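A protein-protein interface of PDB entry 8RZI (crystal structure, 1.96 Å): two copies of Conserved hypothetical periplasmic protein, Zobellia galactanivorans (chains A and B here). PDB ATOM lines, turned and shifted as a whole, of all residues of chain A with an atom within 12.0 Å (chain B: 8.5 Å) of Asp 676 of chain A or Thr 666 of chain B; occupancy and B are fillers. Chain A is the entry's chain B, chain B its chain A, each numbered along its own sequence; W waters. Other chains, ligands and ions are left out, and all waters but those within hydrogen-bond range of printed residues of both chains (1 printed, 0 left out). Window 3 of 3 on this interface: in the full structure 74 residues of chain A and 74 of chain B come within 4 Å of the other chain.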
ATOM      1  N   SER A 672     -21.466  -2.736  -4.559  1.00  0.00           N
ATOM      2  CA  SER A 672     -21.255  -1.526  -5.332  1.00  0.00           C
ATOM      3  C   SER A 672     -20.636  -0.453  -4.461  1.00  0.00           C
ATOM      4  O   SER A 672     -20.818  -0.438  -3.244  1.00  0.00           O
ATOM      5  CB  SER A 672     -22.571  -0.968  -5.873  1.00  0.00           C
ATOM      6  OG  SER A 672     -22.911  -1.609  -7.067  1.00  0.00           O
ATOM      7  N   LEU A 673     -19.975   0.488  -5.116  1.00  0.00           N
ATOM      8  CA  LEU A 673     -19.484   1.691  -4.461  1.00  0.00           C
ATOM      9  C   LEU A 673     -20.214   2.915  -5.016  1.00  0.00           C
ATOM     10  O   LEU A 673     -20.086   3.239  -6.198  1.00  0.00           O
ATOM     11  CB  LEU A 673     -17.978   1.825  -4.654  1.00  0.00           C
ATOM     12  CG  LEU A 673     -17.412   3.147  -4.145  1.00  0.00           C
ATOM     13  CD1 LEU A 673     -17.586   3.243  -2.639  1.00  0.00           C
ATOM     14  CD2 LEU A 673     -15.950   3.201  -4.552  1.00  0.00           C
ATOM     15  N   HIS A 674     -20.990   3.578  -4.167  1.00  0.00           N
ATOM     16  CA  HIS A 674     -21.631   4.821  -4.540  1.00  0.00           C
ATOM     17  C   HIS A 674     -20.708   5.976  -4.169  1.00  0.00           C
ATOM     18  O   HIS A 674     -20.236   6.055  -3.034  1.00  0.00           O
ATOM     19  CB  HIS A 674     -22.972   5.010  -3.833  1.00  0.00           C
ATOM     20  CG  HIS A 674     -23.422   6.433  -3.843  1.00  0.00           C
ATOM     21  ND1 HIS A 674     -23.861   7.060  -4.993  1.00  0.00           N
ATOM     22  CD2 HIS A 674     -23.376   7.393  -2.885  1.00  0.00           C
ATOM     23  CE1 HIS A 674     -24.115   8.336  -4.727  1.00  0.00           C
ATOM     24  NE2 HIS A 674     -23.837   8.561  -3.454  1.00  0.00           N
ATOM     25  N   MET A 675     -20.461   6.866  -5.119  1.00  0.00           N
ATOM     26  CA  MET A 675     -19.613   8.030  -4.888  1.00  0.00           C
ATOM     27  C   MET A 675     -20.403   9.288  -5.225  1.00  0.00           C
ATOM     28  O   MET A 675     -20.804   9.479  -6.374  1.00  0.00           O
ATOM     29  CB  MET A 675     -18.342   7.934  -5.727  1.00  0.00           C
ATOM     30  CG  MET A 675     -17.649   6.591  -5.527  1.00  0.00           C
ATOM     31  SD  MET A 675     -16.104   6.381  -6.446  1.00  0.00           S
ATOM     32  CE  MET A 675     -15.004   7.415  -5.482  1.00  0.00           C
ATOM     33  N   ASP A 676     -20.632  10.134  -4.231  1.00  0.00           N
ATOM     34  CA  ASP A 676     -21.281  11.431  -4.453  1.00  0.00           C
ATOM     35  C   ASP A 676     -20.527  12.267  -5.469  1.00  0.00           C
ATOM     36  O   ASP A 676     -21.150  13.006  -6.253  1.00  0.00           O
ATOM     37  CB  ASP A 676     -21.415  12.202  -3.135  1.00  0.00           C
ATOM     38  CG  ASP A 676     -22.384  11.541  -2.188  1.00  0.00           C
ATOM     39  OD1 ASP A 676     -23.414  11.028  -2.680  1.00  0.00           O
ATOM     40  OD2 ASP A 676     -22.130  11.500  -0.962  1.00  0.00           O
ATOM     41  OXT ASP A 676     -19.286  12.211  -5.548  1.00  0.00           O
ATOM     42  N   LEU B 597     -11.554   4.327  -5.097  1.00  0.00           N
ATOM     43  CA  LEU B 597     -11.669   4.848  -3.739  1.00  0.00           C
ATOM     44  C   LEU B 597     -10.360   4.830  -2.957  1.00  0.00           C
ATOM     45  O   LEU B 597      -9.964   5.859  -2.402  1.00  0.00           O
ATOM     46  CB  LEU B 597     -12.729   4.047  -2.967  1.00  0.00           C
ATOM     47  CG  LEU B 597     -12.929   4.410  -1.485  1.00  0.00           C
ATOM     48  CD1 LEU B 597     -13.418   5.842  -1.345  1.00  0.00           C
ATOM     49  CD2 LEU B 597     -13.910   3.438  -0.816  1.00  0.00           C
ATOM     50  N   ILE B 634     -12.631  10.001   7.354  1.00  0.00           N
ATOM     51  CA  ILE B 634     -13.666   9.507   8.252  1.00  0.00           C
ATOM     52  C   ILE B 634     -14.345   8.323   7.571  1.00  0.00           C
ATOM     53  O   ILE B 634     -14.660   8.387   6.378  1.00  0.00           O
ATOM     54  CB  ILE B 634     -14.681  10.605   8.614  1.00  0.00           C
ATOM     55  CG1 ILE B 634     -13.939  11.821   9.218  1.00  0.00           C
ATOM     56  CG2 ILE B 634     -15.750  10.039   9.578  1.00  0.00           C
ATOM     57  CD1 ILE B 634     -14.835  13.024   9.481  1.00  0.00           C
ATOM     58  N   ILE B 648     -23.106  15.991  11.286  1.00  0.00           N
ATOM     59  CA  ILE B 648     -22.772  15.335  10.029  1.00  0.00           C
ATOM     60  C   ILE B 648     -23.033  13.843  10.179  1.00  0.00           C
ATOM     61  O   ILE B 648     -22.719  13.244  11.214  1.00  0.00           O
ATOM     62  CB  ILE B 648     -21.305  15.599   9.638  1.00  0.00           C
ATOM     63  CG1 ILE B 648     -21.087  17.073   9.319  1.00  0.00           C
ATOM     64  CG2 ILE B 648     -20.903  14.735   8.439  1.00  0.00           C
ATOM     65  CD1 ILE B 648     -19.726  17.351   8.681  1.00  0.00           C
ATOM     66  N   SER B 649     -23.623  13.234   9.155  1.00  0.00           N
ATOM     67  CA  SER B 649     -23.970  11.820   9.182  1.00  0.00           C
ATOM     68  C   SER B 649     -23.012  11.045   8.279  1.00  0.00           C
ATOM     69  O   SER B 649     -22.775  11.445   7.132  1.00  0.00           O
ATOM     70  CB  SER B 649     -25.428  11.622   8.748  1.00  0.00           C
ATOM     71  OG  SER B 649     -25.766  10.251   8.731  1.00  0.00           O
ATOM     72  N   ILE B 650     -22.444   9.966   8.797  1.00  0.00           N
ATOM     73  CA  ILE B 650     -21.590   9.069   8.019  1.00  0.00           C
ATOM     74  C   ILE B 650     -22.389   7.823   7.697  1.00  0.00           C
ATOM     75  O   ILE B 650     -22.783   7.087   8.619  1.00  0.00           O
ATOM     76  CB  ILE B 650     -20.297   8.705   8.770  1.00  0.00           C
ATOM     77  CG1 ILE B 650     -19.628   9.953   9.327  1.00  0.00           C
ATOM     78  CG2 ILE B 650     -19.317   7.961   7.821  1.00  0.00           C
ATOM     79  CD1 ILE B 650     -19.311  10.983   8.288  1.00  0.00           C
ATOM     80  N   PRO B 651     -22.655   7.526   6.427  1.00  0.00           N
ATOM     81  CA  PRO B 651     -23.464   6.366   6.081  1.00  0.00           C
ATOM     82  C   PRO B 651     -22.811   5.073   6.551  1.00  0.00           C
ATOM     83  O   PRO B 651     -21.599   4.997   6.753  1.00  0.00           O
ATOM     84  CB  PRO B 651     -23.535   6.428   4.549  1.00  0.00           C
ATOM     85  CG  PRO B 651     -23.143   7.855   4.196  1.00  0.00           C
ATOM     86  CD  PRO B 651     -22.206   8.288   5.245  1.00  0.00           C
ATOM     87  N   GLY B 654     -19.589   3.673   4.986  1.00  0.00           N
ATOM     88  CA  GLY B 654     -19.519   4.919   4.258  1.00  0.00           C
ATOM     89  C   GLY B 654     -18.291   5.695   4.691  1.00  0.00           C
ATOM     90  O   GLY B 654     -17.591   5.304   5.629  1.00  0.00           O
ATOM     91  N   TYR B 655     -18.044   6.812   4.003  1.00  0.00           N
ATOM     92  CA  TYR B 655     -16.821   7.586   4.188  1.00  0.00           C
ATOM     93  C   TYR B 655     -17.063   9.055   3.866  1.00  0.00           C
ATOM     94  O   TYR B 655     -17.940   9.421   3.064  1.00  0.00           O
ATOM     95  CB  TYR B 655     -15.666   7.064   3.308  1.00  0.00           C
ATOM     96  CG  TYR B 655     -15.993   7.085   1.828  1.00  0.00           C
ATOM     97  CD1 TYR B 655     -15.726   8.206   1.050  1.00  0.00           C
ATOM     98  CD2 TYR B 655     -16.593   5.995   1.212  1.00  0.00           C
ATOM     99  CE1 TYR B 655     -16.045   8.233  -0.311  1.00  0.00           C
ATOM    100  CE2 TYR B 655     -16.924   6.014  -0.152  1.00  0.00           C
ATOM    101  CZ  TYR B 655     -16.646   7.128  -0.899  1.00  0.00           C
ATOM    102  OH  TYR B 655     -16.963   7.165  -2.242  1.00  0.00           O
ATOM    103  N   ARG B 656     -16.231   9.888   4.498  1.00  0.00           N
ATOM    104  CA  ARG B 656     -16.192  11.328   4.285  1.00  0.00           C
ATOM    105  C   ARG B 656     -14.724  11.731   4.346  1.00  0.00           C
ATOM    106  O   ARG B 656     -14.125  11.685   5.424  1.00  0.00           O
ATOM    107  CB  ARG B 656     -17.019  12.060   5.341  1.00  0.00           C
ATOM    108  CG  ARG B 656     -17.002  13.575   5.187  1.00  0.00           C
ATOM    109  CD  ARG B 656     -17.870  14.270   6.251  1.00  0.00           C
ATOM    110  NE  ARG B 656     -18.104  15.688   5.942  1.00  0.00           N
ATOM    111  CZ  ARG B 656     -19.214  16.149   5.362  1.00  0.00           C
ATOM    112  NH1 ARG B 656     -20.189  15.313   5.019  1.00  0.00           N
ATOM    113  NH2 ARG B 656     -19.360  17.447   5.120  1.00  0.00           N
ATOM    114  N   ILE B 657     -14.131  12.077   3.203  1.00  0.00           N
ATOM    115  CA  ILE B 657     -12.673  12.211   3.086  1.00  0.00           C
ATOM    116  C   ILE B 657     -12.315  13.596   2.567  1.00  0.00           C
ATOM    117  O   ILE B 657     -12.671  13.954   1.434  1.00  0.00           O
ATOM    118  CB  ILE B 657     -12.065  11.142   2.166  1.00  0.00           C
ATOM    119  CG1 ILE B 657     -12.398   9.743   2.705  1.00  0.00           C
ATOM    120  CG2 ILE B 657     -10.536  11.352   2.053  1.00  0.00           C
ATOM    121  CD1 ILE B 657     -11.940   8.619   1.830  1.00  0.00           C
ATOM    122  N   GLN B 658     -11.577  14.357   3.370  1.00  0.00           N
ATOM    123  CA  GLN B 658     -11.095  15.676   2.957  1.00  0.00           C
ATOM    124  C   GLN B 658      -9.710  15.501   2.334  1.00  0.00           C
ATOM    125  O   GLN B 658      -8.754  15.129   3.022  1.00  0.00           O
ATOM    126  CB  GLN B 658     -11.076  16.637   4.146  1.00  0.00           C
ATOM    127  CG  GLN B 658     -10.463  18.011   3.864  1.00  0.00           C
ATOM    128  CD  GLN B 658     -11.188  18.794   2.759  1.00  0.00           C
ATOM    129  OE1 GLN B 658     -10.813  18.722   1.583  1.00  0.00           O
ATOM    130  NE2 GLN B 658     -12.220  19.553   3.137  1.00  0.00           N
ATOM    131  N   MET B 659      -9.612  15.720   1.023  1.00  0.00           N
ATOM    132  CA  MET B 659      -8.359  15.561   0.290  1.00  0.00           C
ATOM    133  C   MET B 659      -7.538  16.848   0.359  1.00  0.00           C
ATOM    134  O   MET B 659      -8.064  17.936   0.602  1.00  0.00           O
ATOM    135  CB  MET B 659      -8.625  15.195  -1.178  1.00  0.00           C
ATOM    136  CG  MET B 659      -9.418  13.897  -1.348  1.00  0.00           C
ATOM    137  SD  MET B 659      -8.527  12.440  -0.784  1.00  0.00           S
ATOM    138  CE  MET B 659      -7.200  12.338  -1.985  1.00  0.00           C
ATOM    139  N   SER B 663     -10.996  18.893  -2.257  1.00  0.00           N
ATOM    140  CA  SER B 663     -12.198  18.161  -2.603  1.00  0.00           C
ATOM    141  C   SER B 663     -12.635  17.338  -1.407  1.00  0.00           C
ATOM    142  O   SER B 663     -11.813  16.917  -0.582  1.00  0.00           O
ATOM    143  CB  SER B 663     -11.975  17.254  -3.821  1.00  0.00           C
ATOM    144  OG  SER B 663     -10.905  16.332  -3.627  1.00  0.00           O
ATOM    145  N   LEU B 664     -13.946  17.135  -1.305  1.00  0.00           N
ATOM    146  CA  LEU B 664     -14.544  16.302  -0.267  1.00  0.00           C
ATOM    147  C   LEU B 664     -15.152  15.079  -0.947  1.00  0.00           C
ATOM    148  O   LEU B 664     -16.098  15.210  -1.730  1.00  0.00           O
ATOM    149  CB  LEU B 664     -15.587  17.087   0.524  1.00  0.00           C
ATOM    150  CG  LEU B 664     -16.049  16.362   1.788  1.00  0.00           C
ATOM    151  CD1 LEU B 664     -15.038  16.511   2.906  1.00  0.00           C
ATOM    152  CD2 LEU B 664     -17.426  16.848   2.233  1.00  0.00           C
ATOM    153  N   LYS B 665     -14.594  13.902  -0.671  1.00  0.00           N
ATOM    154  CA  LYS B 665     -15.106  12.651  -1.212  1.00  0.00           C
ATOM    155  C   LYS B 665     -16.080  12.039  -0.214  1.00  0.00           C
ATOM    156  O   LYS B 665     -15.725  11.806   0.950  1.00  0.00           O
ATOM    157  CB  LYS B 665     -13.977  11.664  -1.498  1.00  0.00           C
ATOM    158  CG  LYS B 665     -12.949  12.140  -2.515  1.00  0.00           C
ATOM    159  CD  LYS B 665     -11.908  11.044  -2.691  1.00  0.00           C
ATOM    160  CE  LYS B 665     -11.130  11.202  -3.977  1.00  0.00           C
ATOM    161  NZ  LYS B 665      -9.774  10.611  -3.836  1.00  0.00           N
ATOM    162  N   THR B 666     -17.298  11.771  -0.665  1.00  0.00           N
ATOM    163  CA  THR B 666     -18.281  11.120   0.183  1.00  0.00           C
ATOM    164  C   THR B 666     -18.957  10.014  -0.611  1.00  0.00           C
ATOM    165  O   THR B 666     -19.138  10.115  -1.829  1.00  0.00           O
ATOM    166  CB  THR B 666     -19.340  12.099   0.710  1.00  0.00           C
ATOM    167  OG1 THR B 666     -19.976  12.767  -0.395  1.00  0.00           O
ATOM    168  CG2 THR B 666     -18.715  13.120   1.666  1.00  0.00           C
ATOM    169  N   GLY B 667     -19.348   8.970   0.101  1.00  0.00           N
ATOM    170  CA  GLY B 667     -19.977   7.835  -0.533  1.00  0.00           C
ATOM    171  C   GLY B 667     -20.132   6.713   0.467  1.00  0.00           C
ATOM    172  O   GLY B 667     -19.907   6.895   1.669  1.00  0.00           O
ATOM    173  N   HIS B 668     -20.492   5.546  -0.060  1.00  0.00           N
ATOM    174  CA  HIS B 668     -20.689   4.368   0.776  1.00  0.00           C
ATOM    175  C   HIS B 668     -20.813   3.149  -0.125  1.00  0.00           C
ATOM    176  O   HIS B 668     -21.126   3.267  -1.319  1.00  0.00           O
ATOM    177  CB  HIS B 668     -21.941   4.487   1.662  1.00  0.00           C
ATOM    178  CG  HIS B 668     -23.223   4.437   0.894  1.00  0.00           C
ATOM    179  ND1 HIS B 668     -23.827   5.562   0.370  1.00  0.00           N
ATOM    180  CD2 HIS B 668     -24.017   3.390   0.551  1.00  0.00           C
ATOM    181  CE1 HIS B 668     -24.933   5.213  -0.265  1.00  0.00           C
ATOM    182  NE2 HIS B 668     -25.075   3.902  -0.165  1.00  0.00           N
ATOM    183  N   PHE B 669     -20.521   1.987   0.457  1.00  0.00           N
ATOM    184  CA  PHE B 669     -20.724   0.717  -0.216  1.00  0.00           C
ATOM    185  C   PHE B 669     -22.169   0.269  -0.061  1.00  0.00           C
ATOM    186  O   PHE B 669     -22.818   0.533   0.955  1.00  0.00           O
ATOM    187  CB  PHE B 669     -19.803  -0.359   0.352  1.00  0.00           C
ATOM    188  CG  PHE B 669     -18.349  -0.151   0.027  1.00  0.00           C
ATOM    189  CD1 PHE B 669     -17.812  -0.611  -1.175  1.00  0.00           C
ATOM    190  CD2 PHE B 669     -17.524   0.491   0.919  1.00  0.00           C
ATOM    191  CE1 PHE B 669     -16.459  -0.423  -1.478  1.00  0.00           C
ATOM    192  CE2 PHE B 669     -16.163   0.690   0.623  1.00  0.00           C
ATOM    193  CZ  PHE B 669     -15.637   0.220  -0.581  1.00  0.00           C
HETATM  194  O   HOH W   1     -17.476  12.282  -3.587  1.00  0.00           O
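Printed residues of chain B within 4 Å of Leu 673 of chain A: Leu 597, Tyr 655 and His 668. Of the printed residues of chain B, Met 675 of chain A touches Tyr 655 (3.4 Å) and Thr 666 (3.7 Å). Of chain B, only Thr 666 (2.6 Å) and Gly 667 (3.9 Å) come within 4 Å of Asp 676 of chain A. Of the printed residues of chain A, Leu 597 of chain B touches Leu 673 (3.7 Å). Gly 654 of chain B touches none of the printed residues of chain A. Tyr 655 of chain B touches just these residues of chain A: Leu 673 (3.8 Å), His 674 (3.5 Å) and Met 675 (3.4 Å). No residue of chain A comes within 4 Å of Arg 656 of chain B. Met 659 of chain B touches none of the printed residues of chain A. No residue of chain A comes within 4 Å of Leu 664 of chain B. Thr 666 of chain B touches two residues of chain A. Gly 667 of chain B touches just these residues of chain A: His 674 and Asp 676. Of the printed residues of chain A, Phe 669 of chain B touches Ser 672. The nearest residue of chain B that does not touch Asp 676 of chain A is Tyr 655 of chain B (5.1 Å). The nearest residue of chain A that does not touch Thr 666 of chain B is His 674 of chain A (4.4 Å). The nearest printed residue of chain A that does not touch His 668 of chain B is Ser 672 of chain A (4.2 Å).
No position is printed for both chains. Of the 11 pairs that touch across the chains among the printed residues, none has its exchanged pair printed and touching as well.
Water W1 lies within hydrogen-bond range of the chain-end carboxylate of Asp 676 of chain A (2.7 Å) and the backbone NH of Thr 666 of chain B (3.0 Å).
The side-chain hydroxyl (OG1) of Thr 666 of chain B is in hydrogen-bond range of the side-chain carboxylate (OD2) of Asp 676 of chain A. O of His 668 of chain B lies within hydrogen-bond range of N of His 674 of chain A (2.9 Å).
CA of Phe 669 of chain B touches O of Ser 672 of chain A, at 3.2 Å. Leu 673 of chain A touches Leu 597 of chain B. Leu 673 of chain A touches Tyr 655 of chain B (CD1 to CE2, 3.8 Å). His 668 of chain B touches Leu 673 of chain A. His 674 of chain A touches Tyr 655 of chain B (O to OH, 3.5 Å). O of His 674 of chain A touches CA of Gly 667 of chain B, at 3.1 Å. Tyr 655 of chain B touches Met 675 of chain A (OH to CG, 3.4 Å). Thr 666 of chain B touches Met 675 of chain A. Asp 676 of chain A touches Gly 667 of chain B.
O of Gly 667 of chain B lies within hydrogen-bond range of N of Tyr 655 of chain B, 3.0 Å away. The side-chain carboxylate (OD1) of Asp 676 of chain A sits at hydrogen-bond distance from a ring nitrogen (NE2) of His 674 of chain A, 2.6 Å away.
Printed residues of chain B that touch a printed residue of chain A: Leu 597, Tyr 655, Thr 666, Gly 667, His 668 and Phe 669. Hydrophobic or aromatic side chains of chain B within 4 Å of the printed part of chain A: Leu 597, Tyr 655, His 668 and Phe 669. Of the 5 printed residues of chain A, 5 touch a printed residue of chain B. Along chain A the printed residues that touch a printed residue of chain B span positions 672 to 676. Among the printed residues, 11 pairs touch across the chains. Among the printed residues, no Asp or Glu carboxylate lies within 4 Å of a Lys or Arg side-chain nitrogen of the other chain.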
